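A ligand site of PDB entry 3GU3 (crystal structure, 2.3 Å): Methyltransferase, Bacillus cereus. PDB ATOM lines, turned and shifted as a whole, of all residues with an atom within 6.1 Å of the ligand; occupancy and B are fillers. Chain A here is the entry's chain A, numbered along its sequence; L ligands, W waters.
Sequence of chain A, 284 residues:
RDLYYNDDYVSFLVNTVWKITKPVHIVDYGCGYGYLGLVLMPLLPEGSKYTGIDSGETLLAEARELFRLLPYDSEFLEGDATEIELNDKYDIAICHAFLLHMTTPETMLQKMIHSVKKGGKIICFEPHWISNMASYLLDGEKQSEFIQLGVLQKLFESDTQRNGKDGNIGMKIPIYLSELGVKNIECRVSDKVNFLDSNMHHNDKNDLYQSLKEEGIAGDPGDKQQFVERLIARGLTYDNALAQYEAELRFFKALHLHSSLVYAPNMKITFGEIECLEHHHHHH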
ATOM      1  N   ASP A  28      16.769   4.079  -7.533  1.00  0.00           N
ATOM      2  CA  ASP A  28      17.650   5.182  -7.151  1.00  0.00           C
ATOM      3  C   ASP A  28      18.070   5.086  -5.682  1.00  0.00           C
ATOM      4  O   ASP A  28      17.236   5.219  -4.778  1.00  0.00           O
ATOM      5  CB  ASP A  28      16.923   6.512  -7.407  1.00  0.00           C
ATOM      6  CG  ASP A  28      17.797   7.723  -7.134  1.00  0.00           C
ATOM      7  OD1 ASP A  28      17.248   8.840  -7.046  1.00  0.00           O
ATOM      8  OD2 ASP A  28      19.020   7.559  -7.016  1.00  0.00           O
ATOM      9  N   TYR A  29      19.364   4.867  -5.453  1.00  0.00           N
ATOM     10  CA  TYR A  29      19.903   4.736  -4.100  1.00  0.00           C
ATOM     11  C   TYR A  29      20.229   6.083  -3.450  1.00  0.00           C
ATOM     12  O   TYR A  29      20.917   6.915  -4.038  1.00  0.00           O
ATOM     13  CB  TYR A  29      21.155   3.849  -4.109  1.00  0.00           C
ATOM     14  CG  TYR A  29      20.872   2.401  -4.433  1.00  0.00           C
ATOM     15  CD1 TYR A  29      20.591   1.981  -5.739  1.00  0.00           C
ATOM     16  CD2 TYR A  29      20.908   1.436  -3.424  1.00  0.00           C
ATOM     17  CE1 TYR A  29      20.338   0.633  -6.026  1.00  0.00           C
ATOM     18  CE2 TYR A  29      20.662   0.090  -3.705  1.00  0.00           C
ATOM     19  CZ  TYR A  29      20.381  -0.306  -5.004  1.00  0.00           C
ATOM     20  OH  TYR A  29      20.163  -1.638  -5.275  1.00  0.00           O
ATOM     21  N   GLY A  30      19.752   6.273  -2.224  1.00  0.00           N
ATOM     22  CA  GLY A  30      19.957   7.530  -1.531  1.00  0.00           C
ATOM     23  C   GLY A  30      19.253   8.616  -2.314  1.00  0.00           C
ATOM     24  O   GLY A  30      19.804   9.698  -2.527  1.00  0.00           O
ATOM     25  N   CYS A  31      18.024   8.326  -2.729  1.00  0.00           N
ATOM     26  CA  CYS A  31      17.220   9.242  -3.537  1.00  0.00           C
ATOM     27  C   CYS A  31      16.881  10.584  -2.909  1.00  0.00           C
ATOM     28  O   CYS A  31      16.402  11.486  -3.610  1.00  0.00           O
ATOM     29  CB  CYS A  31      15.910   8.559  -3.916  1.00  0.00           C
ATOM     30  SG  CYS A  31      14.871   8.195  -2.466  1.00  0.00           S
ATOM     31  N   GLY A  32      17.096  10.723  -1.610  1.00  0.00           N
ATOM     32  CA  GLY A  32      16.750  11.979  -0.956  1.00  0.00           C
ATOM     33  C   GLY A  32      15.266  12.203  -1.147  1.00  0.00           C
ATOM     34  O   GLY A  32      14.482  11.290  -0.914  1.00  0.00           O
ATOM     35  N   TYR A  33      14.869  13.401  -1.576  1.00  0.00           N
ATOM     36  CA  TYR A  33      13.455  13.666  -1.798  1.00  0.00           C
ATOM     37  C   TYR A  33      13.018  13.296  -3.227  1.00  0.00           C
ATOM     38  O   TYR A  33      11.943  13.690  -3.668  1.00  0.00           O
ATOM     39  CB  TYR A  33      13.101  15.128  -1.503  1.00  0.00           C
ATOM     40  CG  TYR A  33      13.817  16.170  -2.352  1.00  0.00           C
ATOM     41  CD1 TYR A  33      13.463  16.380  -3.691  1.00  0.00           C
ATOM     42  CD2 TYR A  33      14.873  16.915  -1.814  1.00  0.00           C
ATOM     43  CE1 TYR A  33      14.157  17.309  -4.475  1.00  0.00           C
ATOM     44  CE2 TYR A  33      15.568  17.844  -2.597  1.00  0.00           C
ATOM     45  CZ  TYR A  33      15.213  18.026  -3.926  1.00  0.00           C
ATOM     46  OH  TYR A  33      15.915  18.906  -4.698  1.00  0.00           O
ATOM     47  N   GLY A  34      13.869  12.533  -3.929  1.00  0.00           N
ATOM     48  CA  GLY A  34      13.545  12.103  -5.290  1.00  0.00           C
ATOM     49  C   GLY A  34      14.081  12.969  -6.411  1.00  0.00           C
ATOM     50  O   GLY A  34      13.543  12.969  -7.518  1.00  0.00           O
ATOM     51  N   TYR A  35      15.157  13.701  -6.133  1.00  0.00           N
ATOM     52  CA  TYR A  35      15.765  14.598  -7.115  1.00  0.00           C
ATOM     53  C   TYR A  35      16.012  13.986  -8.496  1.00  0.00           C
ATOM     54  O   TYR A  35      15.521  14.492  -9.508  1.00  0.00           O
ATOM     55  CB  TYR A  35      17.074  15.157  -6.554  1.00  0.00           C
ATOM     56  CG  TYR A  35      17.858  15.979  -7.562  1.00  0.00           C
ATOM     57  CD1 TYR A  35      18.981  15.447  -8.188  1.00  0.00           C
ATOM     58  CD2 TYR A  35      17.449  17.259  -7.916  1.00  0.00           C
ATOM     59  CE1 TYR A  35      19.680  16.171  -9.144  1.00  0.00           C
ATOM     60  CE2 TYR A  35      18.133  17.993  -8.875  1.00  0.00           C
ATOM     61  CZ  TYR A  35      19.249  17.445  -9.487  1.00  0.00           C
ATOM     62  OH  TYR A  35      19.920  18.164 -10.455  1.00  0.00           O
ATOM     63  N   LEU A  36      16.760  12.888  -8.533  1.00  0.00           N
ATOM     64  CA  LEU A  36      17.078  12.264  -9.805  1.00  0.00           C
ATOM     65  C   LEU A  36      15.824  11.804 -10.555  1.00  0.00           C
ATOM     66  O   LEU A  36      15.787  11.818 -11.786  1.00  0.00           O
ATOM     67  CB  LEU A  36      18.039  11.090  -9.588  1.00  0.00           C
ATOM     68  CG  LEU A  36      18.940  10.798 -10.795  1.00  0.00           C
ATOM     69  CD1 LEU A  36      19.605  12.087 -11.253  1.00  0.00           C
ATOM     70  CD2 LEU A  36      19.968   9.766 -10.428  1.00  0.00           C
ATOM     71  N   ILE A  53      15.323   4.747  -2.780  1.00  0.00           N
ATOM     72  CA  ILE A  53      15.681   4.166  -1.488  1.00  0.00           C
ATOM     73  C   ILE A  53      16.375   5.213  -0.637  1.00  0.00           C
ATOM     74  O   ILE A  53      17.275   5.910  -1.100  1.00  0.00           O
ATOM     75  CB  ILE A  53      16.654   2.973  -1.658  1.00  0.00           C
ATOM     76  CG1 ILE A  53      15.996   1.877  -2.498  1.00  0.00           C
ATOM     77  CG2 ILE A  53      17.034   2.391  -0.314  1.00  0.00           C
ATOM     78  CD1 ILE A  53      16.953   0.783  -2.887  1.00  0.00           C
ATOM     79  N   ASP A  54      15.939   5.347   0.610  1.00  0.00           N
ATOM     80  CA  ASP A  54      16.568   6.303   1.503  1.00  0.00           C
ATOM     81  C   ASP A  54      16.230   5.984   2.967  1.00  0.00           C
ATOM     82  O   ASP A  54      15.202   5.374   3.262  1.00  0.00           O
ATOM     83  CB  ASP A  54      16.138   7.723   1.150  1.00  0.00           C
ATOM     84  CG  ASP A  54      17.126   8.759   1.639  1.00  0.00           C
ATOM     85  OD1 ASP A  54      17.277   8.885   2.876  1.00  0.00           O
ATOM     86  OD2 ASP A  54      17.761   9.433   0.802  1.00  0.00           O
ATOM     87  N   SER A  55      17.109   6.396   3.868  1.00  0.00           N
ATOM     88  CA  SER A  55      16.919   6.148   5.295  1.00  0.00           C
ATOM     89  C   SER A  55      16.198   7.292   5.988  1.00  0.00           C
ATOM     90  O   SER A  55      15.674   7.121   7.079  1.00  0.00           O
ATOM     91  CB  SER A  55      18.280   5.927   5.971  1.00  0.00           C
ATOM     92  OG  SER A  55      19.115   7.051   5.815  1.00  0.00           O
ATOM     93  N   GLY A  56      16.174   8.461   5.348  1.00  0.00           N
ATOM     94  CA  GLY A  56      15.508   9.606   5.933  1.00  0.00           C
ATOM     95  C   GLY A  56      14.001   9.542   5.829  1.00  0.00           C
ATOM     96  O   GLY A  56      13.443   9.710   4.742  1.00  0.00           O
ATOM     97  N   LEU A  59      12.539  12.758   4.615  1.00  0.00           N
ATOM     98  CA  LEU A  59      12.863  12.904   3.202  1.00  0.00           C
ATOM     99  C   LEU A  59      11.861  12.138   2.353  1.00  0.00           C
ATOM    100  O   LEU A  59      11.292  12.676   1.398  1.00  0.00           O
ATOM    101  CB  LEU A  59      14.278  12.389   2.907  1.00  0.00           C
ATOM    102  CG  LEU A  59      15.468  13.344   3.099  1.00  0.00           C
ATOM    103  CD1 LEU A  59      15.259  14.584   2.222  1.00  0.00           C
ATOM    104  CD2 LEU A  59      15.594  13.735   4.553  1.00  0.00           C
ATOM    105  N   GLY A  79      14.897   2.513   4.344  1.00  0.00           N
ATOM    106  CA  GLY A  79      15.827   1.522   4.847  1.00  0.00           C
ATOM    107  C   GLY A  79      17.277   1.860   4.545  1.00  0.00           C
ATOM    108  O   GLY A  79      17.554   2.772   3.765  1.00  0.00           O
ATOM    109  N   ASP A  80      18.202   1.144   5.178  1.00  0.00           N
ATOM    110  CA  ASP A  80      19.631   1.346   4.996  1.00  0.00           C
ATOM    111  C   ASP A  80      20.040   0.695   3.681  1.00  0.00           C
ATOM    112  O   ASP A  80      19.966  -0.527   3.533  1.00  0.00           O
ATOM    113  CB  ASP A  80      20.419   0.714   6.159  1.00  0.00           C
ATOM    114  CG  ASP A  80      21.926   0.881   6.027  1.00  0.00           C
ATOM    115  OD1 ASP A  80      22.631   0.589   7.016  1.00  0.00           O
ATOM    116  OD2 ASP A  80      22.409   1.307   4.960  1.00  0.00           O
ATOM    117  N   ALA A  81      20.457   1.516   2.722  1.00  0.00           N
ATOM    118  CA  ALA A  81      20.854   1.044   1.400  1.00  0.00           C
ATOM    119  C   ALA A  81      21.999   0.044   1.458  1.00  0.00           C
ATOM    120  O   ALA A  81      22.178  -0.741   0.521  1.00  0.00           O
ATOM    121  CB  ALA A  81      21.239   2.218   0.526  1.00  0.00           C
ATOM    122  N   THR A  82      22.778   0.074   2.535  1.00  0.00           N
ATOM    123  CA  THR A  82      23.910  -0.854   2.642  1.00  0.00           C
ATOM    124  C   THR A  82      23.486  -2.213   3.170  1.00  0.00           C
ATOM    125  O   THR A  82      24.293  -3.135   3.232  1.00  0.00           O
ATOM    126  CB  THR A  82      25.010  -0.317   3.561  1.00  0.00           C
ATOM    127  OG1 THR A  82      24.539  -0.325   4.915  1.00  0.00           O
ATOM    128  CG2 THR A  82      25.400   1.118   3.179  1.00  0.00           C
ATOM    129  N   CYS A  95      22.125   6.694  -8.913  1.00  0.00           N
ATOM    130  CA  CYS A  95      22.303   7.412  -7.667  1.00  0.00           C
ATOM    131  C   CYS A  95      22.841   8.799  -8.010  1.00  0.00           C
ATOM    132  O   CYS A  95      23.472   8.977  -9.052  1.00  0.00           O
ATOM    133  CB  CYS A  95      23.258   6.684  -6.727  1.00  0.00           C
ATOM    134  SG  CYS A  95      25.002   6.691  -7.194  1.00  0.00           S
ATOM    135  N   HIS A  96      22.565   9.771  -7.143  1.00  0.00           N
ATOM    136  CA  HIS A  96      23.027  11.130  -7.362  1.00  0.00           C
ATOM    137  C   HIS A  96      23.585  11.681  -6.071  1.00  0.00           C
ATOM    138  O   HIS A  96      22.864  11.773  -5.078  1.00  0.00           O
ATOM    139  CB  HIS A  96      21.878  12.030  -7.851  1.00  0.00           C
ATOM    140  CG  HIS A  96      22.317  13.402  -8.232  1.00  0.00           C
ATOM    141  ND1 HIS A  96      22.536  14.405  -7.307  1.00  0.00           N
ATOM    142  CD2 HIS A  96      22.652  13.928  -9.434  1.00  0.00           C
ATOM    143  CE1 HIS A  96      22.986  15.474  -7.922  1.00  0.00           C
ATOM    144  NE2 HIS A  96      23.067  15.220  -9.210  1.00  0.00           N
ATOM    145  N   ALA A  97      24.867  12.022  -6.085  1.00  0.00           N
ATOM    146  CA  ALA A  97      25.573  12.567  -4.923  1.00  0.00           C
ATOM    147  C   ALA A  97      25.299  11.690  -3.717  1.00  0.00           C
ATOM    148  O   ALA A  97      24.943  12.175  -2.642  1.00  0.00           O
ATOM    149  CB  ALA A  97      25.098  13.990  -4.649  1.00  0.00           C
ATOM    150  N   PHE A  98      25.493  10.390  -3.898  1.00  0.00           N
ATOM    151  CA  PHE A  98      25.231   9.423  -2.840  1.00  0.00           C
ATOM    152  C   PHE A  98      26.494   8.695  -2.403  1.00  0.00           C
ATOM    153  O   PHE A  98      26.806   8.643  -1.213  1.00  0.00           O
ATOM    154  CB  PHE A  98      24.187   8.415  -3.340  1.00  0.00           C
ATOM    155  CG  PHE A  98      24.042   7.197  -2.467  1.00  0.00           C
ATOM    156  CD1 PHE A  98      24.361   5.931  -2.950  1.00  0.00           C
ATOM    157  CD2 PHE A  98      23.551   7.308  -1.165  1.00  0.00           C
ATOM    158  CE1 PHE A  98      24.196   4.788  -2.159  1.00  0.00           C
ATOM    159  CE2 PHE A  98      23.385   6.171  -0.361  1.00  0.00           C
ATOM    160  CZ  PHE A  98      23.711   4.907  -0.868  1.00  0.00           C
ATOM    161  N   HIS A 101      29.223   9.796   0.223  1.00  0.00           N
ATOM    162  CA  HIS A 101      28.936   9.718   1.647  1.00  0.00           C
ATOM    163  C   HIS A 101      29.183   8.315   2.208  1.00  0.00           C
ATOM    164  O   HIS A 101      29.077   8.084   3.401  1.00  0.00           O
ATOM    165  CB  HIS A 101      27.484  10.141   1.925  1.00  0.00           C
ATOM    166  CG  HIS A 101      27.152  11.520   1.465  1.00  0.00           C
ATOM    167  ND1 HIS A 101      27.772  12.644   1.955  1.00  0.00           N
ATOM    168  CD2 HIS A 101      26.279  11.960   0.528  1.00  0.00           C
ATOM    169  CE1 HIS A 101      27.296  13.723   1.353  1.00  0.00           C
ATOM    170  NE2 HIS A 101      26.381  13.332   0.482  1.00  0.00           N
ATOM    171  N   MET A 102      29.516   7.379   1.327  1.00  0.00           N
ATOM    172  CA  MET A 102      29.784   6.007   1.716  1.00  0.00           C
ATOM    173  C   MET A 102      31.236   5.848   2.163  1.00  0.00           C
ATOM    174  O   MET A 102      32.147   6.366   1.511  1.00  0.00           O
ATOM    175  CB  MET A 102      29.535   5.051   0.547  1.00  0.00           C
ATOM    176  CG  MET A 102      28.103   5.031   0.054  1.00  0.00           C
ATOM    177  SD  MET A 102      26.897   4.238   1.358  1.00  0.00           S
ATOM    178  CE  MET A 102      26.236   5.865   2.169  1.00  0.00           C
ATOM    179  N   MET A 108      29.191  -0.636  -1.814  1.00  0.00           N
ATOM    180  CA  MET A 108      27.856  -0.131  -2.135  1.00  0.00           C
ATOM    181  C   MET A 108      27.618  -0.245  -3.648  1.00  0.00           C
ATOM    182  O   MET A 108      26.516  -0.574  -4.079  1.00  0.00           O
ATOM    183  CB  MET A 108      27.715   1.323  -1.688  1.00  0.00           C
ATOM    184  CG  MET A 108      26.318   1.882  -1.841  1.00  0.00           C
ATOM    185  SD  MET A 108      24.996   0.933  -0.779  1.00  0.00           S
ATOM    186  CE  MET A 108      23.940   0.128  -2.179  1.00  0.00           C
HETATM  187  N1  LIG L   1      19.713  11.911  -4.841  1.00  0.00           N
HETATM  188  C1  LIG L   1      19.700  12.875  -3.740  1.00  0.00           C
HETATM  189  C2  LIG L   1      20.850  12.521  -2.770  1.00  0.00           C
HETATM  190  C3  LIG L   1      20.972  13.438  -1.538  1.00  0.00           C
HETATM  191  S1  LIG L   1      22.351  13.284  -0.374  1.00  0.00           S
HETATM  192  C4  LIG L   1      19.877  14.318  -4.304  1.00  0.00           C
HETATM  193  O1  LIG L   1      20.734  14.464  -5.231  1.00  0.00           O
HETATM  194  O2  LIG L   1      19.188  15.270  -3.835  1.00  0.00           O
HETATM  195  C5  LIG L   1      22.394  11.434  -0.232  1.00  0.00           C
HETATM  196  C6  LIG L   1      21.284  10.746   0.532  1.00  0.00           C
HETATM  197  O3  LIG L   1      21.887   9.575   1.062  1.00  0.00           O
HETATM  198  C7  LIG L   1      20.627  11.591   1.708  1.00  0.00           C
HETATM  199  O4  LIG L   1      19.256  11.989   1.329  1.00  0.00           O
HETATM  200  C8  LIG L   1      20.700  10.667   2.936  1.00  0.00           C
HETATM  201  O5  LIG L   1      19.428  10.284   3.488  1.00  0.00           O
HETATM  202  C9  LIG L   1      21.578   9.485   2.483  1.00  0.00           C
HETATM  203  N2  LIG L   1      22.159   8.250   2.984  1.00  0.00           N
HETATM  204  C10 LIG L   1      23.414   8.064   3.610  1.00  0.00           C
HETATM  205  N3  LIG L   1      23.597   6.794   3.931  1.00  0.00           N
HETATM  206  C11 LIG L   1      22.450   6.116   3.512  1.00  0.00           C
HETATM  207  C12 LIG L   1      21.966   4.737   3.564  1.00  0.00           C
HETATM  208  N4  LIG L   1      22.698   3.744   4.085  1.00  0.00           N
HETATM  209  N5  LIG L   1      20.715   4.409   3.020  1.00  0.00           N
HETATM  210  C13 LIG L   1      19.970   5.383   2.507  1.00  0.00           C
HETATM  211  N6  LIG L   1      20.283   6.668   2.401  1.00  0.00           N
HETATM  212  C14 LIG L   1      21.527   7.004   2.934  1.00  0.00           C
HETATM  213  O   HOH W   1      20.499   9.011  -5.510  1.00  0.00           O
HETATM  214  O   HOH W   2      17.711  11.371  -6.318  1.00  0.00           O
HETATM  215  O   HOH W   3      16.516  14.737  -3.106  1.00  0.00           O
HETATM  216  O   HOH W   4      24.243   7.116   6.843  1.00  0.00           O
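The side-chain hydroxyl (OG1) of Thr 82 lies within hydrogen-bond range of the side-chain carboxylate (OD2) of Asp 80 (2.7 Å). The backbone NH (N) of Gly 32 is in hydrogen-bond range of the side-chain carboxylate (OD2) of Asp 54, 2.8 Å away. The backbone NH (N) of Gly 79 sits at hydrogen-bond distance from the backbone carbonyl oxygen (O) of Asp 54 (3.1 Å). N of Gly 56 sits at hydrogen-bond distance from OD1 of Asp 54, at 2.7 Å. The backbone NH of Gly 30 lies within hydrogen-bond range of the backbone carbonyl oxygen of Ile 53, at 2.7 Å. The backbone NH of Cys 31 sits at hydrogen-bond distance from the backbone carbonyl oxygen of Ile 53, 3.0 Å away.
N4 of the ligand sits at hydrogen-bond distance from OD2 of Asp 80 (2.6 Å). OD1 of Asp 54 is in hydrogen-bond range of O5 of the ligand. A nitrogen (N1) of the ligand sits close to the backbone carbonyl oxygen (O) of His 96 (3.2 Å). A ring nitrogen (ND1) of His 96 is in hydrogen-bond range of an oxygen (O1) of the ligand, at 2.7 Å. N of Ala 81 lies within hydrogen-bond range of N5 of the ligand, 2.9 Å away. The backbone carbonyl oxygen (O) of Gly 30 sits close to a nitrogen (N1) of the ligand (3.2 Å).
The backbone carbonyl oxygen (O) of Ala 97 sits close to a sulfur (S1) of the ligand (3.6 Å). Residues that only touch the ligand: Cys 31, Gly 32, Tyr 35, Ser 55, Gly 79, Thr 82, Phe 98, His 101 and Met 102. Hydrophobic or aromatic side chains that line the ligand: Tyr 35, Ala 81, His 96, Phe 98, His 101 and Met 102. Of the 25 residues printed, 15 come within 4 Å of the ligand. Along chain A the residues within 4 Å of the ligand span positions 30 to 102. The nearest printed residue that does not touch the ligand is Gly 56 (4.2 Å).
Water W2 lies within hydrogen-bond range of N1 of the ligand (2.5 Å), OD1 of Asp 28 (2.7 Å), N of Leu 36 (2.8 Å), O of Cys 31 (3.0 Å) and N of Tyr 35 (3.5 Å). Water W3 lies within hydrogen-bond range of the backbone NH (N) of Tyr 33 (2.6 Å), an oxygen (O2) of the ligand (2.8 Å), the backbone carbonyl oxygen (O) of Cys 31 (3.3 Å) and the backbone NH (N) of Tyr 35 (3.5 Å).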
